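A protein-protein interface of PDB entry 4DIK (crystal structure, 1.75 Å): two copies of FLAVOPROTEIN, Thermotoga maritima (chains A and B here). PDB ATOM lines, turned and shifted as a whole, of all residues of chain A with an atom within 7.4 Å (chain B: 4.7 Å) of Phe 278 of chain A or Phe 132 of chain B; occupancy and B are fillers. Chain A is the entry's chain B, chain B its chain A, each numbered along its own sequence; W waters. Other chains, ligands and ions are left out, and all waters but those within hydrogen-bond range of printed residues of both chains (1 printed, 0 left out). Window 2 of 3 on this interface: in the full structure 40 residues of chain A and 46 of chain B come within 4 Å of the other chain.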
ATOM      1  N   ASP A 273     -18.359  14.216   9.669  1.00  0.00           N
ATOM      2  CA  ASP A 273     -19.458  14.998   9.143  1.00  0.00           C
ATOM      3  C   ASP A 273     -20.714  14.605   9.900  1.00  0.00           C
ATOM      4  O   ASP A 273     -20.917  13.437  10.230  1.00  0.00           O
ATOM      5  CB  ASP A 273     -19.658  14.718   7.653  1.00  0.00           C
ATOM      6  CG  ASP A 273     -20.452  13.469   7.415  1.00  0.00           C
ATOM      7  OD1 ASP A 273     -19.834  12.394   7.262  1.00  0.00           O
ATOM      8  OD2 ASP A 273     -21.708  13.565   7.437  1.00  0.00           O
ATOM      9  N   SER A 274     -21.559  15.576  10.189  1.00  0.00           N
ATOM     10  CA  SER A 274     -22.848  15.258  10.771  1.00  0.00           C
ATOM     11  C   SER A 274     -23.877  15.981   9.936  1.00  0.00           C
ATOM     12  O   SER A 274     -23.974  17.222  10.004  1.00  0.00           O
ATOM     13  CB  SER A 274     -22.908  15.686  12.242  1.00  0.00           C
ATOM     14  OG  SER A 274     -24.145  15.297  12.813  1.00  0.00           O
ATOM     15  N   MET A 275     -24.600  15.198   9.132  1.00  0.00           N
ATOM     16  CA  MET A 275     -25.638  15.731   8.253  1.00  0.00           C
ATOM     17  C   MET A 275     -26.855  16.209   9.069  1.00  0.00           C
ATOM     18  O   MET A 275     -27.370  17.296   8.782  1.00  0.00           O
ATOM     19  CB  MET A 275     -26.038  14.710   7.145  1.00  0.00           C
ATOM     20  CG  MET A 275     -24.914  14.333   6.153  1.00  0.00           C
ATOM     21  SD  MET A 275     -25.220  13.019   4.919  1.00  0.00           S
ATOM     22  CE  MET A 275     -26.407  13.868   3.867  1.00  0.00           C
ATOM     23  N   TYR A 276     -27.284  15.454  10.100  1.00  0.00           N
ATOM     24  CA  TYR A 276     -28.438  15.864  10.925  1.00  0.00           C
ATOM     25  C   TYR A 276     -28.347  15.662  12.434  1.00  0.00           C
ATOM     26  O   TYR A 276     -29.366  15.714  13.144  1.00  0.00           O
ATOM     27  CB  TYR A 276     -29.724  15.190  10.445  1.00  0.00           C
ATOM     28  CG  TYR A 276     -30.248  15.783   9.172  1.00  0.00           C
ATOM     29  CD1 TYR A 276     -30.852  17.034   9.169  1.00  0.00           C
ATOM     30  CD2 TYR A 276     -30.110  15.106   7.967  1.00  0.00           C
ATOM     31  CE1 TYR A 276     -31.317  17.590   7.999  1.00  0.00           C
ATOM     32  CE2 TYR A 276     -30.577  15.640   6.804  1.00  0.00           C
ATOM     33  CZ  TYR A 276     -31.181  16.885   6.813  1.00  0.00           C
ATOM     34  OH  TYR A 276     -31.635  17.418   5.627  1.00  0.00           O
ATOM     35  N   GLY A 277     -27.148  15.451  12.963  1.00  0.00           N
ATOM     36  CA  GLY A 277     -27.023  15.329  14.410  1.00  0.00           C
ATOM     37  C   GLY A 277     -26.862  13.918  14.965  1.00  0.00           C
ATOM     38  O   GLY A 277     -26.497  13.723  16.129  1.00  0.00           O
ATOM     39  N   PHE A 278     -27.126  12.916  14.146  1.00  0.00           N
ATOM     40  CA  PHE A 278     -26.908  11.542  14.586  1.00  0.00           C
ATOM     41  C   PHE A 278     -25.431  11.184  14.724  1.00  0.00           C
ATOM     42  O   PHE A 278     -25.035  10.516  15.678  1.00  0.00           O
ATOM     43  CB  PHE A 278     -27.609  10.565  13.652  1.00  0.00           C
ATOM     44  CG  PHE A 278     -29.095  10.671  13.698  1.00  0.00           C
ATOM     45  CD1 PHE A 278     -29.815  10.062  14.714  1.00  0.00           C
ATOM     46  CD2 PHE A 278     -29.774  11.406  12.741  1.00  0.00           C
ATOM     47  CE1 PHE A 278     -31.195  10.169  14.762  1.00  0.00           C
ATOM     48  CE2 PHE A 278     -31.145  11.519  12.778  1.00  0.00           C
ATOM     49  CZ  PHE A 278     -31.864  10.902  13.789  1.00  0.00           C
ATOM     50  N   VAL A 279     -24.612  11.600  13.761  1.00  0.00           N
ATOM     51  CA  VAL A 279     -23.179  11.368  13.890  1.00  0.00           C
ATOM     52  C   VAL A 279     -22.666  12.189  15.065  1.00  0.00           C
ATOM     53  O   VAL A 279     -21.894  11.689  15.882  1.00  0.00           O
ATOM     54  CB  VAL A 279     -22.414  11.693  12.599  1.00  0.00           C
ATOM     55  CG1 VAL A 279     -20.880  11.585  12.823  1.00  0.00           C
ATOM     56  CG2 VAL A 279     -22.842  10.737  11.490  1.00  0.00           C
ATOM     57  N   GLU A 280     -23.128  13.433  15.162  1.00  0.00           N
ATOM     58  CA  GLU A 280     -22.733  14.325  16.252  1.00  0.00           C
ATOM     59  C   GLU A 280     -22.923  13.690  17.625  1.00  0.00           C
ATOM     60  O   GLU A 280     -22.074  13.833  18.506  1.00  0.00           O
ATOM     61  CB  GLU A 280     -23.506  15.640  16.185  1.00  0.00           C
ATOM     62  CG  GLU A 280     -23.311  16.534  17.406  1.00  0.00           C
ATOM     63  CD  GLU A 280     -21.873  16.989  17.587  1.00  0.00           C
ATOM     64  OE1 GLU A 280     -21.146  17.141  16.573  1.00  0.00           O
ATOM     65  OE2 GLU A 280     -21.458  17.195  18.752  1.00  0.00           O
ATOM     66  N   ASN A 281     -24.037  12.988  17.802  1.00  0.00           N
ATOM     67  CA  ASN A 281     -24.354  12.428  19.108  1.00  0.00           C
ATOM     68  C   ASN A 281     -23.404  11.317  19.505  1.00  0.00           C
ATOM     69  O   ASN A 281     -23.020  11.207  20.668  1.00  0.00           O
ATOM     70  CB  ASN A 281     -25.807  11.953  19.168  1.00  0.00           C
ATOM     71  CG  ASN A 281     -26.784  13.101  19.149  1.00  0.00           C
ATOM     72  OD1 ASN A 281     -26.393  14.258  19.351  1.00  0.00           O
ATOM     73  ND2 ASN A 281     -28.065  12.803  18.903  1.00  0.00           N
ATOM     74  N   VAL A 282     -23.028  10.496  18.535  1.00  0.00           N
ATOM     75  CA  VAL A 282     -22.042   9.453  18.763  1.00  0.00           C
ATOM     76  C   VAL A 282     -20.654  10.046  19.002  1.00  0.00           C
ATOM     77  O   VAL A 282     -19.936   9.636  19.921  1.00  0.00           O
ATOM     78  CB  VAL A 282     -22.019   8.449  17.602  1.00  0.00           C
ATOM     79  CG1 VAL A 282     -20.807   7.528  17.699  1.00  0.00           C
ATOM     80  CG2 VAL A 282     -23.313   7.631  17.598  1.00  0.00           C
ATOM     81  N   MET A 283     -20.281  11.034  18.190  1.00  0.00           N
ATOM     82  CA  MET A 283     -18.947  11.611  18.313  1.00  0.00           C
ATOM     83  C   MET A 283     -18.779  12.421  19.612  1.00  0.00           C
ATOM     84  O   MET A 283     -17.675  12.483  20.166  1.00  0.00           O
ATOM     85  CB  MET A 283     -18.599  12.447  17.076  1.00  0.00           C
ATOM     86  CG  MET A 283     -18.732  11.674  15.760  1.00  0.00           C
ATOM     87  SD  MET A 283     -17.923  10.044  15.698  1.00  0.00           S
ATOM     88  CE  MET A 283     -16.198  10.530  15.561  1.00  0.00           C
ATOM     89  N   LYS A 284     -19.861  13.018  20.106  1.00  0.00           N
ATOM     90  CA  LYS A 284     -19.803  13.780  21.358  1.00  0.00           C
ATOM     91  C   LYS A 284     -19.440  12.866  22.517  1.00  0.00           C
ATOM     92  O   LYS A 284     -18.625  13.235  23.372  1.00  0.00           O
ATOM     93  CB  LYS A 284     -21.130  14.490  21.631  1.00  0.00           C
ATOM     94  CG  LYS A 284     -21.321  14.949  23.090  1.00  0.00           C
ATOM     95  CD  LYS A 284     -20.483  16.198  23.419  1.00  0.00           C
ATOM     96  CE  LYS A 284     -20.762  16.681  24.859  1.00  0.00           C
ATOM     97  NZ  LYS A 284     -19.996  17.937  25.117  1.00  0.00           N
ATOM     98  N   SER A 328     -20.985   9.742   7.635  1.00  0.00           N
ATOM     99  CA  SER A 328     -22.354   9.515   7.174  1.00  0.00           C
ATOM    100  C   SER A 328     -22.345   8.881   5.791  1.00  0.00           C
ATOM    101  O   SER A 328     -21.523   9.229   4.945  1.00  0.00           O
ATOM    102  CB  SER A 328     -23.139  10.822   7.122  1.00  0.00           C
ATOM    103  OG  SER A 328     -23.304  11.370   8.415  1.00  0.00           O
ATOM    104  N   VAL A 360     -22.384   5.477   9.910  1.00  0.00           N
ATOM    105  CA  VAL A 360     -23.816   5.200   9.800  1.00  0.00           C
ATOM    106  C   VAL A 360     -24.050   4.067   8.805  1.00  0.00           C
ATOM    107  O   VAL A 360     -23.356   3.961   7.799  1.00  0.00           O
ATOM    108  CB  VAL A 360     -24.599   6.459   9.363  1.00  0.00           C
ATOM    109  CG1 VAL A 360     -26.090   6.144   9.220  1.00  0.00           C
ATOM    110  CG2 VAL A 360     -24.390   7.578  10.364  1.00  0.00           C
ATOM    111  N   TRP A 363     -28.267   2.579   3.044  1.00  0.00           N
ATOM    112  CA  TRP A 363     -28.920   1.663   2.123  1.00  0.00           C
ATOM    113  C   TRP A 363     -28.207   1.780   0.780  1.00  0.00           C
ATOM    114  O   TRP A 363     -28.773   1.480  -0.274  1.00  0.00           O
ATOM    115  CB  TRP A 363     -30.415   1.996   2.001  1.00  0.00           C
ATOM    116  CG  TRP A 363     -30.714   3.431   1.633  1.00  0.00           C
ATOM    117  CD1 TRP A 363     -30.728   3.969   0.383  1.00  0.00           C
ATOM    118  CD2 TRP A 363     -31.065   4.493   2.529  1.00  0.00           C
ATOM    119  NE1 TRP A 363     -31.052   5.302   0.441  1.00  0.00           N
ATOM    120  CE2 TRP A 363     -31.265   5.646   1.751  1.00  0.00           C
ATOM    121  CE3 TRP A 363     -31.220   4.580   3.919  1.00  0.00           C
ATOM    122  CZ2 TRP A 363     -31.612   6.875   2.310  1.00  0.00           C
ATOM    123  CZ3 TRP A 363     -31.570   5.803   4.473  1.00  0.00           C
ATOM    124  CH2 TRP A 363     -31.760   6.932   3.670  1.00  0.00           C
ATOM    125  N   ILE A 388     -22.867   3.638  13.622  1.00  0.00           N
ATOM    126  CA  ILE A 388     -23.649   4.729  14.218  1.00  0.00           C
ATOM    127  C   ILE A 388     -25.151   4.543  13.975  1.00  0.00           C
ATOM    128  O   ILE A 388     -25.594   4.467  12.822  1.00  0.00           O
ATOM    129  CB  ILE A 388     -23.245   6.121  13.656  1.00  0.00           C
ATOM    130  CG1 ILE A 388     -21.827   6.505  14.095  1.00  0.00           C
ATOM    131  CG2 ILE A 388     -24.223   7.195  14.117  1.00  0.00           C
ATOM    132  CD1 ILE A 388     -21.239   7.699  13.318  1.00  0.00           C
ATOM    133  N   LYS A 389     -25.917   4.481  15.065  1.00  0.00           N
ATOM    134  CA  LYS A 389     -27.367   4.292  15.015  1.00  0.00           C
ATOM    135  C   LYS A 389     -28.113   5.474  15.633  1.00  0.00           C
ATOM    136  O   LYS A 389     -27.534   6.256  16.381  1.00  0.00           O
ATOM    137  CB  LYS A 389     -27.755   3.019  15.773  1.00  0.00           C
ATOM    138  CG  LYS A 389     -27.172   1.737  15.212  1.00  0.00           C
ATOM    139  CD  LYS A 389     -27.588   0.550  16.081  1.00  0.00           C
ATOM    140  CE  LYS A 389     -27.228  -0.777  15.428  1.00  0.00           C
ATOM    141  NZ  LYS A 389     -27.747  -1.938  16.229  1.00  0.00           N
ATOM    142  N   GLY A 390     -29.411   5.587  15.348  1.00  0.00           N
ATOM    143  CA  GLY A 390     -30.203   6.648  15.941  1.00  0.00           C
ATOM    144  C   GLY A 390     -30.606   6.283  17.358  1.00  0.00           C
ATOM    145  O   GLY A 390     -29.792   6.281  18.287  1.00  0.00           O
ATOM    146  N   SER A 391     -31.884   5.975  17.527  1.00  0.00           N
ATOM    147  CA  SER A 391     -32.390   5.420  18.773  1.00  0.00           C
ATOM    148  C   SER A 391     -31.794   4.035  18.960  1.00  0.00           C
ATOM    149  O   SER A 391     -31.307   3.435  18.007  1.00  0.00           O
ATOM    150  CB  SER A 391     -33.897   5.269  18.676  1.00  0.00           C
ATOM    151  OG  SER A 391     -34.190   4.343  17.648  1.00  0.00           O
ATOM    152  N   ASN A 392     -31.860   3.517  20.181  1.00  0.00           N
ATOM    153  CA  ASN A 392     -31.283   2.213  20.519  1.00  0.00           C
ATOM    154  C   ASN A 392     -29.782   2.069  20.225  1.00  0.00           C
ATOM    155  O   ASN A 392     -29.258   0.955  20.200  1.00  0.00           O
ATOM    156  CB  ASN A 392     -32.105   1.037  19.930  1.00  0.00           C
ATOM    157  CG  ASN A 392     -31.851   0.808  18.438  1.00  0.00           C
ATOM    158  OD1 ASN A 392     -30.791   0.309  18.035  1.00  0.00           O
ATOM    159  ND2 ASN A 392     -32.836   1.169  17.610  1.00  0.00           N
ATOM    160  N   MET A 393     -29.086   3.183  20.005  1.00  0.00           N
ATOM    161  CA  MET A 393     -27.628   3.127  19.854  1.00  0.00           C
ATOM    162  C   MET A 393     -27.017   2.639  21.167  1.00  0.00           C
ATOM    163  O   MET A 393     -27.246   3.236  22.230  1.00  0.00           O
ATOM    164  CB  MET A 393     -27.047   4.497  19.479  1.00  0.00           C
ATOM    165  CG  MET A 393     -25.496   4.595  19.506  1.00  0.00           C
ATOM    166  SD  MET A 393     -24.673   3.661  18.199  1.00  0.00           S
ATOM    167  CE  MET A 393     -22.953   3.765  18.733  1.00  0.00           C
ATOM    168  N   THR B  98     -38.879  10.902   5.530  1.00  0.00           N
ATOM    169  CA  THR B  98     -38.393  10.842   6.914  1.00  0.00           C
ATOM    170  C   THR B  98     -37.082  11.615   7.187  1.00  0.00           C
ATOM    171  O   THR B  98     -36.608  11.642   8.328  1.00  0.00           O
ATOM    172  CB  THR B  98     -38.245   9.369   7.387  1.00  0.00           C
ATOM    173  OG1 THR B  98     -37.200   8.730   6.644  1.00  0.00           O
ATOM    174  CG2 THR B  98     -39.551   8.595   7.196  1.00  0.00           C
ATOM    175  N   PRO B 100     -34.525  14.213   8.398  1.00  0.00           N
ATOM    176  CA  PRO B 100     -34.743  15.052   9.578  1.00  0.00           C
ATOM    177  C   PRO B 100     -35.045  16.518   9.331  1.00  0.00           C
ATOM    178  O   PRO B 100     -35.429  17.173  10.303  1.00  0.00           O
ATOM    179  CB  PRO B 100     -33.433  14.885  10.369  1.00  0.00           C
ATOM    180  CG  PRO B 100     -33.026  13.490  10.050  1.00  0.00           C
ATOM    181  CD  PRO B 100     -33.319  13.373   8.565  1.00  0.00           C
ATOM    182  N   LEU B 128     -37.453   3.638   8.529  1.00  0.00           N
ATOM    183  CA  LEU B 128     -36.621   4.774   8.907  1.00  0.00           C
ATOM    184  C   LEU B 128     -37.121   5.525  10.154  1.00  0.00           C
ATOM    185  O   LEU B 128     -36.315   6.023  10.940  1.00  0.00           O
ATOM    186  CB  LEU B 128     -36.452   5.733   7.726  1.00  0.00           C
ATOM    187  CG  LEU B 128     -35.650   5.186   6.544  1.00  0.00           C
ATOM    188  CD1 LEU B 128     -35.686   6.173   5.362  1.00  0.00           C
ATOM    189  CD2 LEU B 128     -34.191   4.878   6.950  1.00  0.00           C
ATOM    190  N   LEU B 129     -38.435   5.616  10.354  1.00  0.00           N
ATOM    191  CA  LEU B 129     -38.920   6.259  11.579  1.00  0.00           C
ATOM    192  C   LEU B 129     -38.521   5.419  12.793  1.00  0.00           C
ATOM    193  O   LEU B 129     -38.223   5.947  13.865  1.00  0.00           O
ATOM    194  CB  LEU B 129     -40.436   6.459  11.536  1.00  0.00           C
ATOM    195  CG  LEU B 129     -40.953   7.560  10.607  1.00  0.00           C
ATOM    196  CD1 LEU B 129     -42.483   7.527  10.501  1.00  0.00           C
ATOM    197  CD2 LEU B 129     -40.497   8.906  11.130  1.00  0.00           C
ATOM    198  N   GLU B 130     -38.488   4.109  12.610  1.00  0.00           N
ATOM    199  CA  GLU B 130     -37.992   3.229  13.664  1.00  0.00           C
ATOM    200  C   GLU B 130     -36.499   3.458  13.926  1.00  0.00           C
ATOM    201  O   GLU B 130     -36.086   3.617  15.070  1.00  0.00           O
ATOM    202  CB  GLU B 130     -38.241   1.765  13.316  1.00  0.00           C
ATOM    203  CG  GLU B 130     -37.967   0.833  14.489  1.00  0.00           C
ATOM    204  CD  GLU B 130     -38.404  -0.607  14.237  1.00  0.00           C
ATOM    205  OE1 GLU B 130     -39.235  -0.863  13.331  1.00  0.00           O
ATOM    206  OE2 GLU B 130     -37.901  -1.491  14.967  1.00  0.00           O
ATOM    207  N   GLY B 131     -35.699   3.486  12.865  1.00  0.00           N
ATOM    208  CA  GLY B 131     -34.257   3.675  13.000  1.00  0.00           C
ATOM    209  C   GLY B 131     -33.845   5.004  13.613  1.00  0.00           C
ATOM    210  O   GLY B 131     -32.967   5.053  14.470  1.00  0.00           O
ATOM    211  N   PHE B 132     -34.485   6.087  13.176  1.00  0.00           N
ATOM    212  CA  PHE B 132     -34.147   7.432  13.643  1.00  0.00           C
ATOM    213  C   PHE B 132     -34.635   7.700  15.067  1.00  0.00           C
ATOM    214  O   PHE B 132     -33.903   8.238  15.897  1.00  0.00           O
ATOM    215  CB  PHE B 132     -34.767   8.480  12.711  1.00  0.00           C
ATOM    216  CG  PHE B 132     -34.096   8.587  11.363  1.00  0.00           C
ATOM    217  CD1 PHE B 132     -32.734   8.330  11.222  1.00  0.00           C
ATOM    218  CD2 PHE B 132     -34.819   8.984  10.246  1.00  0.00           C
ATOM    219  CE1 PHE B 132     -32.106   8.451   9.980  1.00  0.00           C
ATOM    220  CE2 PHE B 132     -34.208   9.097   8.994  1.00  0.00           C
ATOM    221  CZ  PHE B 132     -32.849   8.832   8.865  1.00  0.00           C
ATOM    222  N   TYR B 133     -35.888   7.326  15.342  1.00  0.00           N
ATOM    223  CA  TYR B 133     -36.572   7.826  16.529  1.00  0.00           C
ATOM    224  C   TYR B 133     -37.139   6.761  17.454  1.00  0.00           C
ATOM    225  O   TYR B 133     -37.592   7.085  18.549  1.00  0.00           O
ATOM    226  CB  TYR B 133     -37.704   8.780  16.130  1.00  0.00           C
ATOM    227  CG  TYR B 133     -37.255   9.893  15.195  1.00  0.00           C
ATOM    228  CD1 TYR B 133     -36.276  10.793  15.585  1.00  0.00           C
ATOM    229  CD2 TYR B 133     -37.835  10.054  13.933  1.00  0.00           C
ATOM    230  CE1 TYR B 133     -35.860  11.828  14.734  1.00  0.00           C
ATOM    231  CE2 TYR B 133     -37.418  11.084  13.068  1.00  0.00           C
ATOM    232  CZ  TYR B 133     -36.437  11.962  13.478  1.00  0.00           C
ATOM    233  OH  TYR B 133     -36.027  12.980  12.633  1.00  0.00           O
ATOM    234  N   GLY B 134     -37.150   5.511  17.011  1.00  0.00           N
ATOM    235  CA  GLY B 134     -37.720   4.446  17.821  1.00  0.00           C
ATOM    236  C   GLY B 134     -39.236   4.392  17.724  1.00  0.00           C
ATOM    237  O   GLY B 134     -39.895   3.667  18.476  1.00  0.00           O
ATOM    238  N   TRP B 164     -35.080   9.765  -1.765  1.00  0.00           N
ATOM    239  CA  TRP B 164     -34.834   8.605  -0.917  1.00  0.00           C
ATOM    240  C   TRP B 164     -35.808   7.490  -1.268  1.00  0.00           C
ATOM    241  O   TRP B 164     -36.807   7.726  -1.955  1.00  0.00           O
ATOM    242  CB  TRP B 164     -35.019   8.966   0.561  1.00  0.00           C
ATOM    243  CG  TRP B 164     -33.818   9.535   1.257  1.00  0.00           C
ATOM    244  CD1 TRP B 164     -32.635   9.945   0.687  1.00  0.00           C
ATOM    245  CD2 TRP B 164     -33.689   9.781   2.664  1.00  0.00           C
ATOM    246  NE1 TRP B 164     -31.785  10.418   1.659  1.00  0.00           N
ATOM    247  CE2 TRP B 164     -32.405  10.332   2.878  1.00  0.00           C
ATOM    248  CE3 TRP B 164     -34.537   9.586   3.764  1.00  0.00           C
ATOM    249  CZ2 TRP B 164     -31.946  10.691   4.150  1.00  0.00           C
ATOM    250  CZ3 TRP B 164     -34.078   9.937   5.029  1.00  0.00           C
ATOM    251  CH2 TRP B 164     -32.800  10.485   5.211  1.00  0.00           C
HETATM  252  O   HOH W   1     -31.248   3.182  15.195  1.00  0.00           O
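The backbone carbonyl oxygen (O) of Glu 130 of chain B sits at hydrogen-bond distance from the side-chain hydroxyl (OG) of Ser 391 of chain A.
The backbone NH (N) of Ser 391 of chain A lies within hydrogen-bond range of the backbone carbonyl oxygen (O) of Gly 131 of chain B, at 3.4 Å.
The backbone NH (N) of Ser 391 of chain A lies within hydrogen-bond range of the backbone carbonyl oxygen (O) of Phe 132 of chain B, at 3.4 Å.
The side-chain hydroxyl (OG) of Ser 391 of chain A is in hydrogen-bond range of the backbone NH (N) of Gly 134 of chain B (3.2 Å).
The backbone NH (N) of Gly 134 of chain B lies within hydrogen-bond range of the backbone carbonyl oxygen (O) of Leu 129 of chain B, at 3.4 Å.
ND2 of Asn 392 of chain A sits close to OG of Ser 391 of chain A (3.5 Å).
Among the printed residues, pairs that only touch across the chains: Tyr 276 of chain A with Pro 100 of chain B (3.5 Å), Phe 278 of chain A with Pro 100 of chain B (3.9 Å), Phe 278 of chain A with Phe 132 of chain B (3.5 Å), Trp 363 of chain A with Leu 128 of chain B (3.7 Å), Trp 363 of chain A with Trp 164 of chain B (3.6 Å), Gly 390 of chain A with Gly 131 of chain B (3.5 Å) and Ser 391 of chain A with Tyr 133 of chain B (3.8 Å).
Asp 273 of chain A touches none of the printed residues of chain B.
Of chain B, only Pro 100 (3.9 Å) and Phe 132 (3.5 Å) come within 4 Å of Phe 278 of chain A.
Val 279 of chain A touches none of the printed residues of chain B.
Printed residues of chain B within 4 Å of Trp 363 of chain A: Leu 128 (3.7 Å) and Trp 164 (3.6 Å).
Of the printed residues of chain A, Pro 100 of chain B touches Tyr 276 (3.5 Å) and Phe 278 (3.9 Å).
Printed residues of chain A within 4 Å of Phe 132 of chain B: Phe 278 and Ser 391.
Printed residues of chain A within 4 Å of Tyr 133 of chain B: Ser 391.
The nearest printed residue of chain A that does not touch Trp 164 of chain B is Tyr 276 of chain A (5.8 Å).
Of the 21 printed residues of chain A, 5 touch a printed residue of chain B.
Hydrophobic or aromatic side chains of chain A that line the printed part of chain B: Tyr 276, Phe 278 and Trp 363.
Among the printed residues, 11 pairs touch across the chains.
No position is printed for both chains.
Water W1 lies within hydrogen-bond range of O of Gly 131 of chain B (2.6 Å), O of Ser 391 of chain A (2.8 Å) and N of Gly 390 of chain A (3.0 Å).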
